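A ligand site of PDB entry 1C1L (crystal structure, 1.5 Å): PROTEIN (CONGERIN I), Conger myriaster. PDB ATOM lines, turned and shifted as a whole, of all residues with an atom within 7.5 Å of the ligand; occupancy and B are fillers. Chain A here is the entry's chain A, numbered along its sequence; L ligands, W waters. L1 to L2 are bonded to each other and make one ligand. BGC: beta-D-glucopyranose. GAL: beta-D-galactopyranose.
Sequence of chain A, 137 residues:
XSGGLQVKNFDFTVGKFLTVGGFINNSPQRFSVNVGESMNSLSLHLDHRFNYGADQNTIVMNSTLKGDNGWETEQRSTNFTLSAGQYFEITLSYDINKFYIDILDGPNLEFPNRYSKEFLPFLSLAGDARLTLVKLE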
ATOM      1  N   ARG A  30      15.347   9.698  12.769  1.00  0.00           N
ATOM      2  CA  ARG A  30      14.839  10.623  13.765  1.00  0.00           C
ATOM      3  C   ARG A  30      13.348  10.435  13.943  1.00  0.00           C
ATOM      4  O   ARG A  30      12.720   9.816  13.075  1.00  0.00           O
ATOM      5  CB  ARG A  30      15.066  12.080  13.327  1.00  0.00           C
ATOM      6  CG  ARG A  30      14.380  12.442  12.003  1.00  0.00           C
ATOM      7  CD  ARG A  30      14.813  13.854  11.665  1.00  0.00           C
ATOM      8  NE  ARG A  30      14.268  14.307  10.399  1.00  0.00           N
ATOM      9  CZ  ARG A  30      13.655  15.479  10.246  1.00  0.00           C
ATOM     10  NH1 ARG A  30      13.478  16.343  11.249  1.00  0.00           N
ATOM     11  NH2 ARG A  30      13.193  15.801   9.045  1.00  0.00           N
ATOM     12  N   SER A  32       9.786  12.733  15.819  1.00  0.00           N
ATOM     13  CA  SER A  32       9.338  13.856  16.612  1.00  0.00           C
ATOM     14  C   SER A  32       7.963  13.678  17.232  1.00  0.00           C
ATOM     15  O   SER A  32       7.102  12.947  16.747  1.00  0.00           O
ATOM     16  CB  SER A  32       9.314  15.100  15.752  1.00  0.00           C
ATOM     17  OG  SER A  32       8.577  14.904  14.549  1.00  0.00           O
ATOM     18  N   ASN A  34       4.937  16.121  18.178  1.00  0.00           N
ATOM     19  CA  ASN A  34       4.426  17.403  17.738  1.00  0.00           C
ATOM     20  C   ASN A  34       3.118  17.731  18.426  1.00  0.00           C
ATOM     21  O   ASN A  34       2.192  16.928  18.347  1.00  0.00           O
ATOM     22  CB  ASN A  34       4.176  17.381  16.237  1.00  0.00           C
ATOM     23  CG  ASN A  34       5.397  16.929  15.482  1.00  0.00           C
ATOM     24  OD1 ASN A  34       6.325  17.706  15.220  1.00  0.00           O
ATOM     25  ND2 ASN A  34       5.500  15.637  15.166  1.00  0.00           N
ATOM     26  N   HIS A  45       7.717  21.089  18.518  1.00  0.00           N
ATOM     27  CA  HIS A  45       8.188  20.021  17.664  1.00  0.00           C
ATOM     28  C   HIS A  45       9.400  19.539  18.431  1.00  0.00           C
ATOM     29  O   HIS A  45      10.348  20.310  18.588  1.00  0.00           O
ATOM     30  CB  HIS A  45       8.600  20.554  16.302  1.00  0.00           C
ATOM     31  CG  HIS A  45       9.382  19.592  15.409  1.00  0.00           C
ATOM     32  ND1 HIS A  45       8.952  18.557  14.719  1.00  0.00           N
ATOM     33  CD2 HIS A  45      10.716  19.738  15.121  1.00  0.00           C
ATOM     34  CE1 HIS A  45       9.952  18.066  14.029  1.00  0.00           C
ATOM     35  NE2 HIS A  45      11.008  18.780  14.288  1.00  0.00           N
ATOM     36  N   LEU A  46       9.416  18.312  18.935  1.00  0.00           N
ATOM     37  CA  LEU A  46      10.509  17.782  19.729  1.00  0.00           C
ATOM     38  C   LEU A  46      11.099  16.656  18.919  1.00  0.00           C
ATOM     39  O   LEU A  46      10.518  15.566  18.826  1.00  0.00           O
ATOM     40  CB  LEU A  46       9.961  17.279  21.065  1.00  0.00           C
ATOM     41  CG  LEU A  46      10.925  16.493  21.965  1.00  0.00           C
ATOM     42  CD1 LEU A  46      12.015  17.397  22.489  1.00  0.00           C
ATOM     43  CD2 LEU A  46      10.153  15.861  23.097  1.00  0.00           C
ATOM     44  N   ASP A  47      12.255  16.909  18.301  1.00  0.00           N
ATOM     45  CA  ASP A  47      12.869  15.966  17.380  1.00  0.00           C
ATOM     46  C   ASP A  47      14.097  15.271  17.978  1.00  0.00           C
ATOM     47  O   ASP A  47      15.041  15.935  18.415  1.00  0.00           O
ATOM     48  CB  ASP A  47      13.235  16.742  16.110  1.00  0.00           C
ATOM     49  CG  ASP A  47      13.378  15.904  14.858  1.00  0.00           C
ATOM     50  OD1 ASP A  47      12.804  14.825  14.738  1.00  0.00           O
ATOM     51  OD2 ASP A  47      14.076  16.347  13.965  1.00  0.00           O
ATOM     52  N   ARG A  49      17.052  13.202  17.015  1.00  0.00           N
ATOM     53  CA  ARG A  49      17.795  12.840  15.826  1.00  0.00           C
ATOM     54  C   ARG A  49      18.932  11.906  16.202  1.00  0.00           C
ATOM     55  O   ARG A  49      19.873  12.268  16.921  1.00  0.00           O
ATOM     56  CB  ARG A  49      18.362  14.098  15.162  1.00  0.00           C
ATOM     57  CG  ARG A  49      17.282  15.090  14.781  1.00  0.00           C
ATOM     58  CD  ARG A  49      17.887  16.322  14.158  1.00  0.00           C
ATOM     59  NE  ARG A  49      16.807  17.130  13.651  1.00  0.00           N
ATOM     60  CZ  ARG A  49      16.913  18.263  12.979  1.00  0.00           C
ATOM     61  NH1 ARG A  49      18.102  18.792  12.725  1.00  0.00           N
ATOM     62  NH2 ARG A  49      15.811  18.889  12.567  1.00  0.00           N
ATOM     63  N   TYR A  52      21.320  11.535  11.635  1.00  0.00           N
ATOM     64  CA  TYR A  52      20.729  12.441  10.692  1.00  0.00           C
ATOM     65  C   TYR A  52      21.803  13.394  10.219  1.00  0.00           C
ATOM     66  O   TYR A  52      21.874  14.563  10.601  1.00  0.00           O
ATOM     67  CB  TYR A  52      19.573  13.148  11.405  1.00  0.00           C
ATOM     68  CG  TYR A  52      18.768  14.040  10.486  1.00  0.00           C
ATOM     69  CD1 TYR A  52      18.016  13.460   9.465  1.00  0.00           C
ATOM     70  CD2 TYR A  52      18.752  15.418  10.675  1.00  0.00           C
ATOM     71  CE1 TYR A  52      17.247  14.257   8.632  1.00  0.00           C
ATOM     72  CE2 TYR A  52      17.997  16.234   9.836  1.00  0.00           C
ATOM     73  CZ  TYR A  52      17.245  15.631   8.824  1.00  0.00           C
ATOM     74  OH  TYR A  52      16.437  16.407   8.017  1.00  0.00           O
ATOM     75  N   ASP A  55      23.781  15.843  12.453  1.00  0.00           N
ATOM     76  CA  ASP A  55      23.149  15.656  13.745  1.00  0.00           C
ATOM     77  C   ASP A  55      23.143  14.201  14.113  1.00  0.00           C
ATOM     78  O   ASP A  55      22.516  13.353  13.465  1.00  0.00           O
ATOM     79  CB  ASP A  55      21.729  16.179  13.680  1.00  0.00           C
ATOM     80  CG  ASP A  55      21.696  17.686  13.612  1.00  0.00           C
ATOM     81  OD1 ASP A  55      22.583  18.341  14.178  1.00  0.00           O
ATOM     82  OD2 ASP A  55      20.791  18.213  12.989  1.00  0.00           O
ATOM     83  N   VAL A  60      16.391  18.421  18.924  1.00  0.00           N
ATOM     84  CA  VAL A  60      16.110  19.711  18.333  1.00  0.00           C
ATOM     85  C   VAL A  60      14.670  20.050  18.690  1.00  0.00           C
ATOM     86  O   VAL A  60      13.763  19.251  18.444  1.00  0.00           O
ATOM     87  CB  VAL A  60      16.266  19.663  16.800  1.00  0.00           C
ATOM     88  CG1 VAL A  60      15.868  21.004  16.189  1.00  0.00           C
ATOM     89  CG2 VAL A  60      17.715  19.350  16.429  1.00  0.00           C
ATOM     90  N   MET A  61      14.453  21.229  19.236  1.00  0.00           N
ATOM     91  CA  MET A  61      13.132  21.727  19.577  1.00  0.00           C
ATOM     92  C   MET A  61      12.878  22.988  18.781  1.00  0.00           C
ATOM     93  O   MET A  61      13.761  23.845  18.612  1.00  0.00           O
ATOM     94  CB  MET A  61      13.062  22.052  21.057  1.00  0.00           C
ATOM     95  CG  MET A  61      13.189  20.806  21.916  1.00  0.00           C
ATOM     96  SD  MET A  61      13.211  21.222  23.664  1.00  0.00           S
ATOM     97  CE  MET A  61      14.955  21.529  23.833  1.00  0.00           C
ATOM     98  N   ASN A  62      11.654  23.106  18.277  1.00  0.00           N
ATOM     99  CA  ASN A  62      11.285  24.275  17.511  1.00  0.00           C
ATOM    100  C   ASN A  62       9.765  24.360  17.468  1.00  0.00           C
ATOM    101  O   ASN A  62       9.080  23.513  18.061  1.00  0.00           O
ATOM    102  CB  ASN A  62      11.855  24.139  16.101  1.00  0.00           C
ATOM    103  CG  ASN A  62      12.122  25.482  15.445  1.00  0.00           C
ATOM    104  OD1 ASN A  62      11.667  26.538  15.897  1.00  0.00           O
ATOM    105  ND2 ASN A  62      12.835  25.496  14.337  1.00  0.00           N
ATOM    106  N   SER A  63       9.243  25.363  16.770  1.00  0.00           N
ATOM    107  CA  SER A  63       7.842  25.577  16.523  1.00  0.00           C
ATOM    108  C   SER A  63       7.710  26.123  15.096  1.00  0.00           C
ATOM    109  O   SER A  63       8.707  26.451  14.433  1.00  0.00           O
ATOM    110  CB  SER A  63       7.321  26.594  17.538  1.00  0.00           C
ATOM    111  OG  SER A  63       7.930  27.865  17.389  1.00  0.00           O
ATOM    112  N   ASP A  68       6.314  23.264   7.231  1.00  0.00           N
ATOM    113  CA  ASP A  68       7.724  23.101   6.921  1.00  0.00           C
ATOM    114  C   ASP A  68       8.407  24.384   6.445  1.00  0.00           C
ATOM    115  O   ASP A  68       9.631  24.441   6.392  1.00  0.00           O
ATOM    116  CB  ASP A  68       7.859  22.007   5.873  1.00  0.00           C
ATOM    117  CG  ASP A  68       9.264  21.447   5.788  1.00  0.00           C
ATOM    118  OD1 ASP A  68       9.891  21.185   6.812  1.00  0.00           O
ATOM    119  OD2 ASP A  68       9.763  21.277   4.667  1.00  0.00           O
ATOM    120  N   ASN A  69       7.652  25.417   6.110  1.00  0.00           N
ATOM    121  CA  ASN A  69       8.298  26.663   5.705  1.00  0.00           C
ATOM    122  C   ASN A  69       8.300  27.712   6.796  1.00  0.00           C
ATOM    123  O   ASN A  69       8.577  28.882   6.534  1.00  0.00           O
ATOM    124  CB  ASN A  69       7.631  27.202   4.440  1.00  0.00           C
ATOM    125  CG  ASN A  69       8.029  26.306   3.286  1.00  0.00           C
ATOM    126  OD1 ASN A  69       9.194  26.051   2.996  1.00  0.00           O
ATOM    127  ND2 ASN A  69       7.067  25.657   2.657  1.00  0.00           N
ATOM    128  N   GLY A  70       7.993  27.360   8.047  1.00  0.00           N
ATOM    129  CA  GLY A  70       7.970  28.380   9.082  1.00  0.00           C
ATOM    130  C   GLY A  70       8.807  28.020  10.278  1.00  0.00           C
ATOM    131  O   GLY A  70       8.576  28.610  11.329  1.00  0.00           O
ATOM    132  N   TRP A  71       9.718  27.052  10.226  1.00  0.00           N
ATOM    133  CA  TRP A  71      10.523  26.675  11.384  1.00  0.00           C
ATOM    134  C   TRP A  71      11.284  27.880  11.891  1.00  0.00           C
ATOM    135  O   TRP A  71      11.873  28.612  11.087  1.00  0.00           O
ATOM    136  CB  TRP A  71      11.497  25.567  11.040  1.00  0.00           C
ATOM    137  CG  TRP A  71      10.817  24.275  10.625  1.00  0.00           C
ATOM    138  CD1 TRP A  71      10.948  23.777   9.359  1.00  0.00           C
ATOM    139  CD2 TRP A  71      10.025  23.489  11.421  1.00  0.00           C
ATOM    140  NE1 TRP A  71      10.250  22.667   9.352  1.00  0.00           N
ATOM    141  CE2 TRP A  71       9.694  22.449  10.556  1.00  0.00           C
ATOM    142  CE3 TRP A  71       9.577  23.498  12.744  1.00  0.00           C
ATOM    143  CZ2 TRP A  71       8.870  21.410  11.009  1.00  0.00           C
ATOM    144  CZ3 TRP A  71       8.762  22.462  13.193  1.00  0.00           C
ATOM    145  CH2 TRP A  71       8.414  21.415  12.336  1.00  0.00           C
ATOM    146  N   GLU A  72      11.255  28.075  13.200  1.00  0.00           N
ATOM    147  CA  GLU A  72      11.841  29.255  13.785  1.00  0.00           C
ATOM    148  C   GLU A  72      13.198  28.961  14.431  1.00  0.00           C
ATOM    149  O   GLU A  72      13.956  28.144  13.898  1.00  0.00           O
ATOM    150  CB  GLU A  72      10.824  29.806  14.780  1.00  0.00           C
ATOM    151  CG  GLU A  72       9.472  30.145  14.158  1.00  0.00           C
ATOM    152  CD  GLU A  72       8.538  30.944  15.042  1.00  0.00           C
ATOM    153  OE1 GLU A  72       8.989  31.521  16.021  1.00  0.00           O
ATOM    154  OE2 GLU A  72       7.350  31.001  14.735  1.00  0.00           O
ATOM    155  N   THR A  73      13.570  29.604  15.548  1.00  0.00           N
ATOM    156  CA  THR A  73      14.829  29.322  16.215  1.00  0.00           C
ATOM    157  C   THR A  73      14.861  27.973  16.923  1.00  0.00           C
ATOM    158  O   THR A  73      14.071  27.671  17.800  1.00  0.00           O
ATOM    159  CB  THR A  73      15.105  30.450  17.237  1.00  0.00           C
ATOM    160  OG1 THR A  73      15.081  31.661  16.486  1.00  0.00           O
ATOM    161  CG2 THR A  73      16.444  30.296  17.983  1.00  0.00           C
ATOM    162  N   GLU A  74      15.785  27.127  16.489  1.00  0.00           N
ATOM    163  CA  GLU A  74      15.996  25.848  17.143  1.00  0.00           C
ATOM    164  C   GLU A  74      16.686  26.016  18.482  1.00  0.00           C
ATOM    165  O   GLU A  74      17.502  26.913  18.701  1.00  0.00           O
ATOM    166  CB  GLU A  74      16.893  24.953  16.306  1.00  0.00           C
ATOM    167  CG  GLU A  74      16.271  24.651  14.962  1.00  0.00           C
ATOM    168  CD  GLU A  74      17.082  23.690  14.111  1.00  0.00           C
ATOM    169  OE1 GLU A  74      18.271  23.525  14.329  1.00  0.00           O
ATOM    170  OE2 GLU A  74      16.501  23.097  13.215  1.00  0.00           O
ATOM    171  N   GLN A  75      16.251  25.183  19.434  1.00  0.00           N
ATOM    172  CA  GLN A  75      16.955  24.993  20.672  1.00  0.00           C
ATOM    173  C   GLN A  75      17.345  23.521  20.614  1.00  0.00           C
ATOM    174  O   GLN A  75      16.584  22.641  20.242  1.00  0.00           O
ATOM    175  CB  GLN A  75      16.056  25.286  21.867  1.00  0.00           C
ATOM    176  CG  GLN A  75      15.764  26.784  21.908  1.00  0.00           C
ATOM    177  CD  GLN A  75      15.289  27.275  23.270  1.00  0.00           C
ATOM    178  OE1 GLN A  75      15.482  26.585  24.261  1.00  0.00           O
ATOM    179  NE2 GLN A  75      14.738  28.466  23.388  1.00  0.00           N
ATOM    180  N   ARG A  76      18.625  23.259  20.860  1.00  0.00           N
ATOM    181  CA  ARG A  76      19.227  21.942  20.757  1.00  0.00           C
ATOM    182  C   ARG A  76      19.766  21.470  22.073  1.00  0.00           C
ATOM    183  O   ARG A  76      20.142  22.280  22.935  1.00  0.00           O
ATOM    184  CB  ARG A  76      20.366  21.948  19.759  1.00  0.00           C
ATOM    185  CG  ARG A  76      19.847  22.167  18.362  1.00  0.00           C
ATOM    186  CD  ARG A  76      20.954  22.483  17.383  1.00  0.00           C
ATOM    187  NE  ARG A  76      20.408  22.430  16.047  1.00  0.00           N
ATOM    188  CZ  ARG A  76      20.723  21.428  15.232  1.00  0.00           C
ATOM    189  NH1 ARG A  76      21.549  20.477  15.638  1.00  0.00           N
ATOM    190  NH2 ARG A  76      20.174  21.340  14.022  1.00  0.00           N
HETATM  191  C2  BGC L   1      18.791  23.179  10.521  1.00  0.00           C
HETATM  192  C3  BGC L   1      17.947  21.896  10.428  1.00  0.00           C
HETATM  193  C4  BGC L   1      16.600  22.222   9.806  1.00  0.00           C
HETATM  194  C5  BGC L   1      16.814  22.905   8.451  1.00  0.00           C
HETATM  195  C6  BGC L   1      15.513  23.279   7.761  1.00  0.00           C
HETATM  196  C1  BGC L   1      18.889  23.867   9.166  1.00  0.00           C
HETATM  197  O1  BGC L   1      19.516  25.068   9.298  1.00  0.00           O
HETATM  198  O2  BGC L   1      20.086  22.840  10.982  1.00  0.00           O
HETATM  199  O3  BGC L   1      17.760  21.351  11.719  1.00  0.00           O
HETATM  200  O4  BGC L   1      15.845  20.988   9.612  1.00  0.00           O
HETATM  201  O5  BGC L   1      17.561  24.114   8.658  1.00  0.00           O
HETATM  202  O6  BGC L   1      14.740  24.165   8.559  1.00  0.00           O
HETATM  203  C1  GAL L   2      14.502  21.025   9.923  1.00  0.00           C
HETATM  204  C2  GAL L   2      13.838  19.699   9.543  1.00  0.00           C
HETATM  205  C3  GAL L   2      12.383  19.671  10.018  1.00  0.00           C
HETATM  206  C4  GAL L   2      12.299  20.021  11.516  1.00  0.00           C
HETATM  207  C5  GAL L   2      13.058  21.314  11.794  1.00  0.00           C
HETATM  208  C6  GAL L   2      13.090  21.659  13.263  1.00  0.00           C
HETATM  209  O2  GAL L   2      13.884  19.558   8.130  1.00  0.00           O
HETATM  210  O3  GAL L   2      11.859  18.381   9.786  1.00  0.00           O
HETATM  211  O4  GAL L   2      12.855  18.953  12.267  1.00  0.00           O
HETATM  212  O5  GAL L   2      14.425  21.223  11.334  1.00  0.00           O
HETATM  213  O6  GAL L   2      13.743  22.888  13.482  1.00  0.00           O
HETATM  214  O   HOH W   1      14.794  24.750  11.656  1.00  0.00           O
HETATM  215  O   HOH W   2      14.177  26.917   8.298  1.00  0.00           O
HETATM  216  O   HOH W   3       9.863  18.800   8.058  1.00  0.00           O
HETATM  217  O   HOH W   4      16.769  26.220   6.319  1.00  0.00           O
HETATM  218  O   HOH W   5      12.616  21.330   6.305  1.00  0.00           O
HETATM  219  O   HOH W   6       9.986  16.459  10.886  1.00  0.00           O
HETATM  220  O   HOH W   7      16.477  18.984   7.715  1.00  0.00           O
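The side-chain carboxylate of Glu 74 lies within hydrogen-bond range of an oxygen (O3) of BGC L1, 2.6 Å away. A ring nitrogen (NE2) of His 45 is in hydrogen-bond range of an oxygen (O4) of GAL L2, 2.7 Å away. The guanidinium group (NH1) of Arg 49 sits at hydrogen-bond distance from an oxygen (O3) of BGC L1 (2.8 Å). An oxygen (O4) of GAL L2 lies within hydrogen-bond range of the guanidinium group (NH1) of Arg 30, at 2.9 Å. The side-chain amide nitrogen of Asn 62 is in hydrogen-bond range of an oxygen (O6) of GAL L2 (2.9 Å). O3 of BGC L1 lies within hydrogen-bond range of NH2 of Arg 76. The side-chain carboxylate of Asp 47 is in hydrogen-bond range of an oxygen (O4) of GAL L2 (3.3 Å).
N of His 45 sits at hydrogen-bond distance from O of Asn 62 (2.8 Å). ND1 of His 45 is in hydrogen-bond range of OD1 of Asn 34. The guanidinium group (NE) of Arg 49 is in salt-bridge range of the side-chain carboxylate (OD2) of Asp 47. The guanidinium group (NH2) of Arg 30 is in hydrogen-bond range of the side-chain hydroxyl (OH) of Tyr 52, 3.5 Å away. OD1 of Asn 62 sits close to O of Thr 73, 3.3 Å away. The guanidinium group (NH1) of Arg 76 is in salt-bridge range of the side-chain carboxylate (OD1) of Asp 55 (2.8 Å). The backbone NH (N) of Asp 47 sits at hydrogen-bond distance from the backbone carbonyl oxygen (O) of Val 60 (2.8 Å). NE1 of Trp 71 lies within hydrogen-bond range of OD1 of Asp 68 (3.0 Å).
Val 60 touches the ligand. CE2 of Trp 71 touches C4 of GAL L2, at 3.7 Å. Hydrophobic or aromatic side chains within 4 Å of the ligand: His 45, Val 60 and Trp 71. Of the 22 residues printed, 9 come within 4 Å of the ligand.
Water W3 bridges an oxygen (O3) of GAL L2 and the side-chain carboxylate of Asp 68. Water W7 lies within hydrogen-bond range of OH of Tyr 52 (2.6 Å) and O2 of GAL L2 (2.7 Å). Water W1 lies within hydrogen-bond range of O6 of GAL L2, OE2 of Glu 74 and ND2 of Asn 62. Water W5 lies within hydrogen-bond range of the side-chain carboxylate of Asp 68 (2.8 Å) and an oxygen (O2) of GAL L2 (2.8 Å).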
